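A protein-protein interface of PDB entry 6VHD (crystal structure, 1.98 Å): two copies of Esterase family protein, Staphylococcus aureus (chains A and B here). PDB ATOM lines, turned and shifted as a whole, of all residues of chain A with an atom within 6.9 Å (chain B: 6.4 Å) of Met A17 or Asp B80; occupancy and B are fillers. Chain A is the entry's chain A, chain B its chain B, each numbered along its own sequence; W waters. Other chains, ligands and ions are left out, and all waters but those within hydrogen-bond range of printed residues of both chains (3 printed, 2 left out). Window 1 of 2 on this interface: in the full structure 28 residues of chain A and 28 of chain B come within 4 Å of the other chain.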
ATOM      1  N   ASN A   9     -33.372 -13.146  -2.334  1.00  0.00           N
ATOM      2  CA  ASN A   9     -32.377 -12.530  -1.461  1.00  0.00           C
ATOM      3  C   ASN A   9     -31.760 -13.653  -0.648  1.00  0.00           C
ATOM      4  O   ASN A   9     -32.453 -14.271   0.169  1.00  0.00           O
ATOM      5  CB  ASN A   9     -33.005 -11.470  -0.552  1.00  0.00           C
ATOM      6  CG  ASN A   9     -31.975 -10.790   0.354  1.00  0.00           C
ATOM      7  OD1 ASN A   9     -31.201 -11.450   1.058  1.00  0.00           O
ATOM      8  ND2 ASN A   9     -31.962  -9.467   0.334  1.00  0.00           N
ATOM      9  N   TYR A  10     -30.466 -13.915  -0.862  1.00  0.00           N
ATOM     10  CA  TYR A  10     -29.769 -14.971  -0.136  1.00  0.00           C
ATOM     11  C   TYR A  10     -28.412 -14.469   0.363  1.00  0.00           C
ATOM     12  O   TYR A  10     -27.847 -13.510  -0.167  1.00  0.00           O
ATOM     13  CB  TYR A  10     -29.608 -16.232  -1.016  1.00  0.00           C
ATOM     14  CG  TYR A  10     -28.537 -16.151  -2.082  1.00  0.00           C
ATOM     15  CD1 TYR A  10     -28.830 -15.701  -3.358  1.00  0.00           C
ATOM     16  CD2 TYR A  10     -27.234 -16.548  -1.812  1.00  0.00           C
ATOM     17  CE1 TYR A  10     -27.843 -15.634  -4.341  1.00  0.00           C
ATOM     18  CE2 TYR A  10     -26.241 -16.482  -2.776  1.00  0.00           C
ATOM     19  CZ  TYR A  10     -26.548 -16.026  -4.041  1.00  0.00           C
ATOM     20  OH  TYR A  10     -25.550 -15.969  -4.996  1.00  0.00           O
ATOM     21  N   HIS A  11     -27.893 -15.121   1.402  1.00  0.00           N
ATOM     22  CA  HIS A  11     -26.573 -14.797   1.936  1.00  0.00           C
ATOM     23  C   HIS A  11     -25.505 -15.422   1.046  1.00  0.00           C
ATOM     24  O   HIS A  11     -25.374 -16.643   0.999  1.00  0.00           O
ATOM     25  CB  HIS A  11     -26.414 -15.302   3.368  1.00  0.00           C
ATOM     26  CG  HIS A  11     -25.203 -14.753   4.057  1.00  0.00           C
ATOM     27  ND1 HIS A  11     -23.923 -14.982   3.603  1.00  0.00           N
ATOM     28  CD2 HIS A  11     -25.076 -13.993   5.171  1.00  0.00           C
ATOM     29  CE1 HIS A  11     -23.058 -14.383   4.400  1.00  0.00           C
ATOM     30  NE2 HIS A  11     -23.732 -13.774   5.360  1.00  0.00           N
ATOM     31  N   SER A  12     -24.713 -14.599   0.371  1.00  0.00           N
ATOM     32  CA  SER A  12     -23.727 -15.104  -0.585  1.00  0.00           C
ATOM     33  C   SER A  12     -22.429 -15.484   0.120  1.00  0.00           C
ATOM     34  O   SER A  12     -21.827 -14.628   0.779  1.00  0.00           O
ATOM     35  CB  SER A  12     -23.418 -14.068  -1.635  1.00  0.00           C
ATOM     36  OG  SER A  12     -22.216 -14.422  -2.289  1.00  0.00           O
ATOM     37  N   PRO A  13     -21.963 -16.722   0.000  1.00  0.00           N
ATOM     38  CA  PRO A  13     -20.649 -17.044   0.577  1.00  0.00           C
ATOM     39  C   PRO A  13     -19.511 -16.307  -0.097  1.00  0.00           C
ATOM     40  O   PRO A  13     -18.496 -16.045   0.553  1.00  0.00           O
ATOM     41  CB  PRO A  13     -20.535 -18.567   0.385  1.00  0.00           C
ATOM     42  CG  PRO A  13     -21.576 -18.929  -0.612  1.00  0.00           C
ATOM     43  CD  PRO A  13     -22.659 -17.901  -0.536  1.00  0.00           C
ATOM     44  N   THR A  14     -19.660 -15.913  -1.365  1.00  0.00           N
ATOM     45  CA  THR A  14     -18.564 -15.236  -2.045  1.00  0.00           C
ATOM     46  C   THR A  14     -18.414 -13.788  -1.591  1.00  0.00           C
ATOM     47  O   THR A  14     -17.286 -13.311  -1.414  1.00  0.00           O
ATOM     48  CB  THR A  14     -18.750 -15.280  -3.566  1.00  0.00           C
ATOM     49  OG1 THR A  14     -18.788 -16.635  -3.999  1.00  0.00           O
ATOM     50  CG2 THR A  14     -17.580 -14.572  -4.264  1.00  0.00           C
ATOM     51  N   ILE A  15     -19.505 -13.029  -1.457  1.00  0.00           N
ATOM     52  CA  ILE A  15     -19.320 -11.618  -1.091  1.00  0.00           C
ATOM     53  C   ILE A  15     -19.633 -11.335   0.374  1.00  0.00           C
ATOM     54  O   ILE A  15     -19.604 -10.168   0.788  1.00  0.00           O
ATOM     55  CB  ILE A  15     -20.135 -10.670  -1.994  1.00  0.00           C
ATOM     56  CG1 ILE A  15     -21.621 -11.033  -1.949  1.00  0.00           C
ATOM     57  CG2 ILE A  15     -19.600 -10.676  -3.435  1.00  0.00           C
ATOM     58  CD1 ILE A  15     -22.454 -10.100  -2.823  1.00  0.00           C
ATOM     59  N   GLY A  16     -19.940 -12.353   1.166  1.00  0.00           N
ATOM     60  CA  GLY A  16     -20.104 -12.169   2.601  1.00  0.00           C
ATOM     61  C   GLY A  16     -21.282 -11.321   3.054  1.00  0.00           C
ATOM     62  O   GLY A  16     -21.176 -10.626   4.076  1.00  0.00           O
ATOM     63  N   MET A  17     -22.415 -11.386   2.351  1.00  0.00           N
ATOM     64  CA  MET A  17     -23.565 -10.557   2.720  1.00  0.00           C
ATOM     65  C   MET A  17     -24.817 -11.037   1.985  1.00  0.00           C
ATOM     66  O   MET A  17     -24.744 -11.727   0.958  1.00  0.00           O
ATOM     67  CB  MET A  17     -23.304  -9.070   2.458  1.00  0.00           C
ATOM     68  CG  MET A  17     -23.142  -8.731   1.015  1.00  0.00           C
ATOM     69  SD  MET A  17     -22.915  -6.968   0.815  1.00  0.00           S
ATOM     70  CE  MET A  17     -22.606  -6.932  -0.957  1.00  0.00           C
ATOM     71  N   HIS A  18     -25.971 -10.730   2.574  1.00  0.00           N
ATOM     72  CA  HIS A  18     -27.229 -10.868   1.844  1.00  0.00           C
ATOM     73  C   HIS A  18     -27.236  -9.925   0.651  1.00  0.00           C
ATOM     74  O   HIS A  18     -26.743  -8.797   0.729  1.00  0.00           O
ATOM     75  CB  HIS A  18     -28.421 -10.569   2.752  1.00  0.00           C
ATOM     76  CG  HIS A  18     -28.726 -11.663   3.723  1.00  0.00           C
ATOM     77  ND1 HIS A  18     -28.011 -11.850   4.890  1.00  0.00           N
ATOM     78  CD2 HIS A  18     -29.662 -12.638   3.694  1.00  0.00           C
ATOM     79  CE1 HIS A  18     -28.507 -12.887   5.545  1.00  0.00           C
ATOM     80  NE2 HIS A  18     -29.506 -13.384   4.839  1.00  0.00           N
ATOM     81  N   GLN A  19     -27.807 -10.392  -0.458  1.00  0.00           N
ATOM     82  CA  GLN A  19     -27.807  -9.638  -1.705  1.00  0.00           C
ATOM     83  C   GLN A  19     -29.052 -10.027  -2.480  1.00  0.00           C
ATOM     84  O   GLN A  19     -29.461 -11.190  -2.444  1.00  0.00           O
ATOM     85  CB  GLN A  19     -26.557  -9.955  -2.539  1.00  0.00           C
ATOM     86  CG  GLN A  19     -26.313  -9.028  -3.737  1.00  0.00           C
ATOM     87  CD  GLN A  19     -25.522  -7.770  -3.376  1.00  0.00           C
ATOM     88  OE1 GLN A  19     -25.589  -7.276  -2.247  1.00  0.00           O
ATOM     89  NE2 GLN A  19     -24.782  -7.242  -4.340  1.00  0.00           N
ATOM     90  N   ASN A  78     -26.989  -8.052  -8.923  1.00  0.00           N
ATOM     91  CA  ASN A  78     -26.581  -6.700  -8.527  1.00  0.00           C
ATOM     92  C   ASN A  78     -25.106  -6.684  -8.124  1.00  0.00           C
ATOM     93  O   ASN A  78     -24.689  -7.489  -7.280  1.00  0.00           O
ATOM     94  CB  ASN A  78     -27.431  -6.198  -7.366  1.00  0.00           C
ATOM     95  CG  ASN A  78     -26.960  -4.848  -6.845  1.00  0.00           C
ATOM     96  OD1 ASN A  78     -26.464  -4.005  -7.601  1.00  0.00           O
ATOM     97  ND2 ASN A  78     -27.108  -4.639  -5.547  1.00  0.00           N
ATOM     98  N   ASP A  80     -23.364  -3.316  -7.803  1.00  0.00           N
ATOM     99  CA  ASP A  80     -22.961  -2.025  -7.241  1.00  0.00           C
ATOM    100  C   ASP A  80     -22.086  -1.208  -8.204  1.00  0.00           C
ATOM    101  O   ASP A  80     -22.395  -1.108  -9.398  1.00  0.00           O
ATOM    102  CB  ASP A  80     -22.229  -2.286  -5.917  1.00  0.00           C
ATOM    103  CG  ASP A  80     -22.332  -1.146  -4.947  1.00  0.00           C
ATOM    104  OD1 ASP A  80     -23.288  -1.146  -4.137  1.00  0.00           O
ATOM    105  OD2 ASP A  80     -21.443  -0.267  -4.979  1.00  0.00           O
ATOM    106  N   HIS A  91     -15.632  -5.904  -2.830  1.00  0.00           N
ATOM    107  CA  HIS A  91     -16.134  -7.269  -2.888  1.00  0.00           C
ATOM    108  C   HIS A  91     -15.586  -8.014  -4.100  1.00  0.00           C
ATOM    109  O   HIS A  91     -15.144  -7.406  -5.087  1.00  0.00           O
ATOM    110  CB  HIS A  91     -17.669  -7.285  -2.928  1.00  0.00           C
ATOM    111  CG  HIS A  91     -18.303  -6.786  -1.670  1.00  0.00           C
ATOM    112  ND1 HIS A  91     -18.506  -7.595  -0.570  1.00  0.00           N
ATOM    113  CD2 HIS A  91     -18.790  -5.569  -1.338  1.00  0.00           C
ATOM    114  CE1 HIS A  91     -19.096  -6.897   0.383  1.00  0.00           C
ATOM    115  NE2 HIS A  91     -19.287  -5.665  -0.059  1.00  0.00           N
ATOM    116  N   TYR A  93     -16.612  -9.341  -6.804  1.00  0.00           N
ATOM    117  CA  TYR A  93     -17.802  -9.334  -7.647  1.00  0.00           C
ATOM    118  C   TYR A  93     -17.624 -10.106  -8.948  1.00  0.00           C
ATOM    119  O   TYR A  93     -18.623 -10.495  -9.557  1.00  0.00           O
ATOM    120  CB  TYR A  93     -18.227  -7.895  -7.925  1.00  0.00           C
ATOM    121  CG  TYR A  93     -19.196  -7.357  -6.884  1.00  0.00           C
ATOM    122  CD1 TYR A  93     -20.413  -7.976  -6.663  1.00  0.00           C
ATOM    123  CD2 TYR A  93     -18.876  -6.243  -6.109  1.00  0.00           C
ATOM    124  CE1 TYR A  93     -21.303  -7.492  -5.711  1.00  0.00           C
ATOM    125  CE2 TYR A  93     -19.765  -5.738  -5.167  1.00  0.00           C
ATOM    126  CZ  TYR A  93     -20.977  -6.369  -4.973  1.00  0.00           C
ATOM    127  OH  TYR A  93     -21.878  -5.887  -4.042  1.00  0.00           O
ATOM    128  N   TYR A  96     -18.440 -13.403  -7.780  1.00  0.00           N
ATOM    129  CA  TYR A  96     -19.873 -13.425  -7.462  1.00  0.00           C
ATOM    130  C   TYR A  96     -20.718 -13.805  -8.677  1.00  0.00           C
ATOM    131  O   TYR A  96     -21.663 -14.597  -8.556  1.00  0.00           O
ATOM    132  CB  TYR A  96     -20.328 -12.075  -6.901  1.00  0.00           C
ATOM    133  CG  TYR A  96     -21.814 -12.026  -6.550  1.00  0.00           C
ATOM    134  CD1 TYR A  96     -22.345 -12.879  -5.590  1.00  0.00           C
ATOM    135  CD2 TYR A  96     -22.669 -11.117  -7.170  1.00  0.00           C
ATOM    136  CE1 TYR A  96     -23.713 -12.843  -5.242  1.00  0.00           C
ATOM    137  CE2 TYR A  96     -24.029 -11.053  -6.834  1.00  0.00           C
ATOM    138  CZ  TYR A  96     -24.547 -11.931  -5.876  1.00  0.00           C
ATOM    139  OH  TYR A  96     -25.886 -11.884  -5.544  1.00  0.00           O
ATOM    140  N   GLN B  19     -30.858   1.804  -4.732  1.00  0.00           N
ATOM    141  CA  GLN B  19     -30.641   1.122  -3.458  1.00  0.00           C
ATOM    142  C   GLN B  19     -32.002   0.791  -2.856  1.00  0.00           C
ATOM    143  O   GLN B  19     -32.928   1.600  -2.946  1.00  0.00           O
ATOM    144  CB  GLN B  19     -29.831   2.022  -2.498  1.00  0.00           C
ATOM    145  CG  GLN B  19     -29.280   1.322  -1.249  1.00  0.00           C
ATOM    146  CD  GLN B  19     -27.967   0.608  -1.510  1.00  0.00           C
ATOM    147  OE1 GLN B  19     -27.672   0.202  -2.642  1.00  0.00           O
ATOM    148  NE2 GLN B  19     -27.174   0.430  -0.457  1.00  0.00           N
ATOM    149  N   HIS B  48     -28.684  -2.422  10.359  1.00  0.00           N
ATOM    150  CA  HIS B  48     -28.299  -3.831  10.369  1.00  0.00           C
ATOM    151  C   HIS B  48     -26.797  -3.997  10.669  1.00  0.00           C
ATOM    152  O   HIS B  48     -26.013  -3.056  10.582  1.00  0.00           O
ATOM    153  CB  HIS B  48     -28.640  -4.474   9.015  1.00  0.00           C
ATOM    154  CG  HIS B  48     -27.861  -3.894   7.871  1.00  0.00           C
ATOM    155  ND1 HIS B  48     -26.532  -4.201   7.640  1.00  0.00           N
ATOM    156  CD2 HIS B  48     -28.218  -3.019   6.898  1.00  0.00           C
ATOM    157  CE1 HIS B  48     -26.107  -3.543   6.574  1.00  0.00           C
ATOM    158  NE2 HIS B  48     -27.108  -2.813   6.110  1.00  0.00           N
ATOM    159  N   GLY B  49     -26.410  -5.228  11.024  1.00  0.00           N
ATOM    160  CA  GLY B  49     -25.020  -5.568  11.253  1.00  0.00           C
ATOM    161  C   GLY B  49     -24.324  -6.015   9.979  1.00  0.00           C
ATOM    162  O   GLY B  49     -24.896  -6.045   8.891  1.00  0.00           O
ATOM    163  N   LEU B  50     -23.053  -6.362  10.128  1.00  0.00           N
ATOM    164  CA  LEU B  50     -22.269  -6.787   8.981  1.00  0.00           C
ATOM    165  C   LEU B  50     -22.822  -8.103   8.446  1.00  0.00           C
ATOM    166  O   LEU B  50     -23.161  -9.004   9.216  1.00  0.00           O
ATOM    167  CB  LEU B  50     -20.803  -6.951   9.377  1.00  0.00           C
ATOM    168  CG  LEU B  50     -19.816  -7.275   8.266  1.00  0.00           C
ATOM    169  CD1 LEU B  50     -19.716  -6.069   7.371  1.00  0.00           C
ATOM    170  CD2 LEU B  50     -18.465  -7.592   8.869  1.00  0.00           C
ATOM    171  N   SER B  51     -22.934  -8.191   7.121  1.00  0.00           N
ATOM    172  CA  SER B  51     -23.446  -9.305   6.327  1.00  0.00           C
ATOM    173  C   SER B  51     -24.979  -9.295   6.226  1.00  0.00           C
ATOM    174  O   SER B  51     -25.529 -10.046   5.416  1.00  0.00           O
ATOM    175  CB  SER B  51     -22.974 -10.689   6.824  1.00  0.00           C
ATOM    176  OG  SER B  51     -23.791 -11.188   7.876  1.00  0.00           O
ATOM    177  N   SER B  52     -25.682  -8.472   6.998  1.00  0.00           N
ATOM    178  CA  SER B  52     -27.125  -8.338   6.872  1.00  0.00           C
ATOM    179  C   SER B  52     -27.466  -7.249   5.855  1.00  0.00           C
ATOM    180  O   SER B  52     -26.584  -6.607   5.268  1.00  0.00           O
ATOM    181  CB  SER B  52     -27.737  -8.018   8.230  1.00  0.00           C
ATOM    182  OG  SER B  52     -27.770  -9.170   9.044  1.00  0.00           O
ATOM    183  N   ASP B  53     -28.761  -7.020   5.647  1.00  0.00           N
ATOM    184  CA  ASP B  53     -29.179  -5.973   4.713  1.00  0.00           C
ATOM    185  C   ASP B  53     -30.561  -5.470   5.129  1.00  0.00           C
ATOM    186  O   ASP B  53     -30.995  -5.691   6.265  1.00  0.00           O
ATOM    187  CB  ASP B  53     -29.095  -6.474   3.256  1.00  0.00           C
ATOM    188  CG  ASP B  53     -30.215  -7.429   2.864  1.00  0.00           C
ATOM    189  OD1 ASP B  53     -31.095  -7.771   3.690  1.00  0.00           O
ATOM    190  OD2 ASP B  53     -30.205  -7.841   1.679  1.00  0.00           O
ATOM    191  N   ASN B  78     -29.937  -0.072   3.832  1.00  0.00           N
ATOM    192  CA  ASN B  78     -28.872  -1.013   3.521  1.00  0.00           C
ATOM    193  C   ASN B  78     -27.556  -0.255   3.323  1.00  0.00           C
ATOM    194  O   ASN B  78     -27.500   0.679   2.519  1.00  0.00           O
ATOM    195  CB  ASN B  78     -29.230  -1.804   2.254  1.00  0.00           C
ATOM    196  CG  ASN B  78     -28.120  -2.771   1.832  1.00  0.00           C
ATOM    197  OD1 ASN B  78     -27.413  -3.337   2.678  1.00  0.00           O
ATOM    198  ND2 ASN B  78     -27.964  -2.961   0.525  1.00  0.00           N
ATOM    199  N   VAL B  79     -26.486  -0.664   4.020  1.00  0.00           N
ATOM    200  CA  VAL B  79     -25.197   0.010   3.817  1.00  0.00           C
ATOM    201  C   VAL B  79     -24.053  -0.964   3.550  1.00  0.00           C
ATOM    202  O   VAL B  79     -22.875  -0.588   3.668  1.00  0.00           O
ATOM    203  CB  VAL B  79     -24.817   0.929   5.004  1.00  0.00           C
ATOM    204  CG1 VAL B  79     -25.946   1.894   5.361  1.00  0.00           C
ATOM    205  CG2 VAL B  79     -24.370   0.103   6.212  1.00  0.00           C
ATOM    206  N   ASP B  80     -24.361  -2.214   3.203  1.00  0.00           N
ATOM    207  CA  ASP B  80     -23.305  -3.107   2.661  1.00  0.00           C
ATOM    208  C   ASP B  80     -22.249  -3.371   3.749  1.00  0.00           C
ATOM    209  O   ASP B  80     -22.616  -3.624   4.908  1.00  0.00           O
ATOM    210  CB  ASP B  80     -22.798  -2.448   1.381  1.00  0.00           C
ATOM    211  CG  ASP B  80     -22.014  -3.388   0.514  1.00  0.00           C
ATOM    212  OD1 ASP B  80     -22.545  -3.822  -0.531  1.00  0.00           O
ATOM    213  OD2 ASP B  80     -20.860  -3.692   0.882  1.00  0.00           O
ATOM    214  N   HIS B  81     -20.949  -3.310   3.435  1.00  0.00           N
ATOM    215  CA  HIS B  81     -19.872  -3.579   4.392  1.00  0.00           C
ATOM    216  C   HIS B  81     -19.209  -2.291   4.900  1.00  0.00           C
ATOM    217  O   HIS B  81     -18.023  -2.300   5.280  1.00  0.00           O
ATOM    218  CB  HIS B  81     -18.826  -4.498   3.748  1.00  0.00           C
ATOM    219  CG  HIS B  81     -19.181  -5.957   3.778  1.00  0.00           C
ATOM    220  ND1 HIS B  81     -18.262  -6.951   3.522  1.00  0.00           N
ATOM    221  CD2 HIS B  81     -20.354  -6.590   4.038  1.00  0.00           C
ATOM    222  CE1 HIS B  81     -18.847  -8.134   3.632  1.00  0.00           C
ATOM    223  NE2 HIS B  81     -20.117  -7.943   3.941  1.00  0.00           N
ATOM    224  N   SER B  82     -19.963  -1.188   4.921  1.00  0.00           N
ATOM    225  CA  SER B  82     -19.412   0.159   5.042  1.00  0.00           C
ATOM    226  C   SER B  82     -19.090   0.597   6.466  1.00  0.00           C
ATOM    227  O   SER B  82     -18.431   1.623   6.635  1.00  0.00           O
ATOM    228  CB  SER B  82     -20.396   1.174   4.477  1.00  0.00           C
ATOM    229  OG  SER B  82     -21.503   1.275   5.341  1.00  0.00           O
ATOM    230  N   ALA B  83     -19.611  -0.081   7.484  1.00  0.00           N
ATOM    231  CA  ALA B  83     -19.531   0.382   8.865  1.00  0.00           C
ATOM    232  C   ALA B  83     -20.146   1.777   9.049  1.00  0.00           C
ATOM    233  O   ALA B  83     -19.802   2.484  10.005  1.00  0.00           O
ATOM    234  CB  ALA B  83     -18.086   0.362   9.378  1.00  0.00           C
ATOM    235  N   MET B  87     -16.859   6.178   3.035  1.00  0.00           N
ATOM    236  CA  MET B  87     -15.729   5.267   2.869  1.00  0.00           C
ATOM    237  C   MET B  87     -14.570   5.919   2.134  1.00  0.00           C
ATOM    238  O   MET B  87     -14.760   6.696   1.193  1.00  0.00           O
ATOM    239  CB  MET B  87     -16.153   4.011   2.109  1.00  0.00           C
ATOM    240  CG  MET B  87     -17.223   3.182   2.838  1.00  0.00           C
ATOM    241  SD  MET B  87     -18.027   1.930   1.801  1.00  0.00           S
ATOM    242  CE  MET B  87     -16.667   0.769   1.579  1.00  0.00           C
ATOM    243  N   TYR B  93     -21.587   6.440   2.780  1.00  0.00           N
ATOM    244  CA  TYR B  93     -22.696   5.804   3.481  1.00  0.00           C
ATOM    245  C   TYR B  93     -23.088   6.518   4.772  1.00  0.00           C
ATOM    246  O   TYR B  93     -24.243   6.385   5.196  1.00  0.00           O
ATOM    247  CB  TYR B  93     -22.368   4.333   3.759  1.00  0.00           C
ATOM    248  CG  TYR B  93     -22.812   3.407   2.643  1.00  0.00           C
ATOM    249  CD1 TYR B  93     -24.148   3.369   2.237  1.00  0.00           C
ATOM    250  CD2 TYR B  93     -21.903   2.577   1.984  1.00  0.00           C
ATOM    251  CE1 TYR B  93     -24.570   2.520   1.208  1.00  0.00           C
ATOM    252  CE2 TYR B  93     -22.320   1.709   0.961  1.00  0.00           C
ATOM    253  CZ  TYR B  93     -23.662   1.707   0.577  1.00  0.00           C
ATOM    254  OH  TYR B  93     -24.114   0.867  -0.422  1.00  0.00           O
ATOM    255  N   MET B 124     -22.236  -4.180  13.829  1.00  0.00           N
ATOM    256  CA  MET B 124     -21.871  -3.024  13.017  1.00  0.00           C
ATOM    257  C   MET B 124     -22.936  -1.933  13.079  1.00  0.00           C
ATOM    258  O   MET B 124     -22.608  -0.744  13.022  1.00  0.00           O
ATOM    259  CB  MET B 124     -21.634  -3.468  11.572  1.00  0.00           C
ATOM    260  CG  MET B 124     -21.072  -2.385  10.635  1.00  0.00           C
ATOM    261  SD  MET B 124     -20.980  -2.900   8.896  1.00  0.00           S
ATOM    262  CE  MET B 124     -22.705  -2.781   8.402  1.00  0.00           C
ATOM    263  N   TRP B 160     -13.435 -11.115   8.535  1.00  0.00           N
ATOM    264  CA  TRP B 160     -14.733 -11.564   8.045  1.00  0.00           C
ATOM    265  C   TRP B 160     -14.724 -11.816   6.538  1.00  0.00           C
ATOM    266  O   TRP B 160     -14.009 -11.152   5.785  1.00  0.00           O
ATOM    267  CB  TRP B 160     -15.810 -10.538   8.385  1.00  0.00           C
ATOM    268  CG  TRP B 160     -17.183 -10.963   7.976  1.00  0.00           C
ATOM    269  CD1 TRP B 160     -17.831 -10.672   6.798  1.00  0.00           C
ATOM    270  CD2 TRP B 160     -18.077 -11.776   8.733  1.00  0.00           C
ATOM    271  NE1 TRP B 160     -19.077 -11.245   6.789  1.00  0.00           N
ATOM    272  CE2 TRP B 160     -19.254 -11.928   7.966  1.00  0.00           C
ATOM    273  CE3 TRP B 160     -18.003 -12.382   9.989  1.00  0.00           C
ATOM    274  CZ2 TRP B 160     -20.346 -12.666   8.421  1.00  0.00           C
ATOM    275  CZ3 TRP B 160     -19.088 -13.109  10.438  1.00  0.00           C
ATOM    276  CH2 TRP B 160     -20.242 -13.248   9.657  1.00  0.00           C
ATOM    277  N   ASN B 161     -15.570 -12.753   6.100  1.00  0.00           N
ATOM    278  CA  ASN B 161     -15.761 -13.089   4.685  1.00  0.00           C
ATOM    279  C   ASN B 161     -15.875 -11.864   3.771  1.00  0.00           C
ATOM    280  O   ASN B 161     -16.814 -11.077   3.912  1.00  0.00           O
ATOM    281  CB  ASN B 161     -17.027 -13.931   4.526  1.00  0.00           C
ATOM    282  CG  ASN B 161     -17.053 -14.697   3.228  1.00  0.00           C
ATOM    283  OD1 ASN B 161     -16.178 -14.531   2.375  1.00  0.00           O
ATOM    284  ND2 ASN B 161     -18.081 -15.524   3.052  1.00  0.00           N
HETATM  285  O   HOH W   1     -28.541  -6.438  -0.073  1.00  0.00           O
HETATM  286  O   HOH W   2     -22.292  -0.702  -1.628  1.00  0.00           O
HETATM  287  O   HOH W   3     -21.246  -3.831  -2.904  1.00  0.00           O
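N of Ile A15 is in hydrogen-bond range of OG of Ser A12, at 3.2 Å. The backbone carbonyl oxygen (O) of Met A17 lies within hydrogen-bond range of the backbone NH (N) of Ser A12. A ring nitrogen (ND1) of His A91 is in hydrogen-bond range of the backbone carbonyl oxygen (O) of Ile A15 (3.1 Å). OD1 of Asn B78 lies within hydrogen-bond range of N of Asp B80 (3.3 Å).
4 positions are printed for both chains. Of the 15 pairs that touch across the chains among the printed residues, none has its exchanged pair printed and touching as well.
Printed residues of chain A that touch a printed residue of chain B: Asn A9, His A11, Pro A13, Ile A15, Gly A16, Met A17, His A18 and His A91. Hydrophobic or aromatic side chains of chain B that line the printed part of chain A: His B81 and Trp B160.
ND2 of Asn A9 is in hydrogen-bond range of OD2 of Asp B53. O of Pro A13 lies within hydrogen-bond range of ND2 of Asn B161. The backbone carbonyl oxygen (O) of Gly A16 lies within hydrogen-bond range of a ring nitrogen (NE2) of His B81 (2.9 Å). NE1 of Trp B160 sits at hydrogen-bond distance from O of Gly A16, at 3.5 Å. The backbone carbonyl oxygen (O) of Ser B51 sits at hydrogen-bond distance from the backbone NH (N) of His A18, 3.0 Å away. A ring nitrogen (NE2) of His A91 lies within hydrogen-bond range of the side-chain carboxylate (OD2) of Asp B80, at 2.7 Å. The side-chain sulfur of Met A17 sits close to the side-chain carboxylate of Asp B80, 3.4 Å away.
NE2 of His A11 touches CB of Ser B51, at 3.5 Å. Ile A15 touches His B81. O of Gly A16 touches CB of Ser B51 (3.3 Å). Gly A16 touches Asn B161 (CA to O, 3.7 Å). O of Ser B51 touches CA of Met A17 (3.4 Å). His B81 touches Met A17 (NE2 to CB, 3.7 Å). CB of His A18 touches OD2 of Asp B53, 3.4 Å away. His A91 touches His B81 (CE1 to ND1, 3.2 Å).
Met A17 touches three residues of chain B. Printed residues of chain A within 4 Å of Trp B160: Gly A16 (3.5 Å). Of the printed residues of chain B, Pro A13 touches Asn B161 (2.6 Å). Of the printed residues of chain A, Asn B161 touches Pro A13 (2.6 Å) and Gly A16 (3.7 Å). Thr A14 touches none of the printed residues of chain B. The nearest residue of chain B that does not touch Met A17 is Ser B52 (5.0 Å). The nearest printed residue of chain B that does not touch His A91 is Asn B161 (5.9 Å).
Water W3 lies within hydrogen-bond range of the side-chain hydroxyl (OH) of Tyr A93 and the side-chain carboxylate (OD1) of Asp B80. Water W2 lies within hydrogen-bond range of the side-chain hydroxyl of Tyr B93 (2.7 Å), the side-chain carboxylate of Asp A80 (2.7 Å) and the side-chain carboxylate of Asp B80 (3.3 Å). Water W1 bridges OD2 of Asp B53 and O of His A18.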
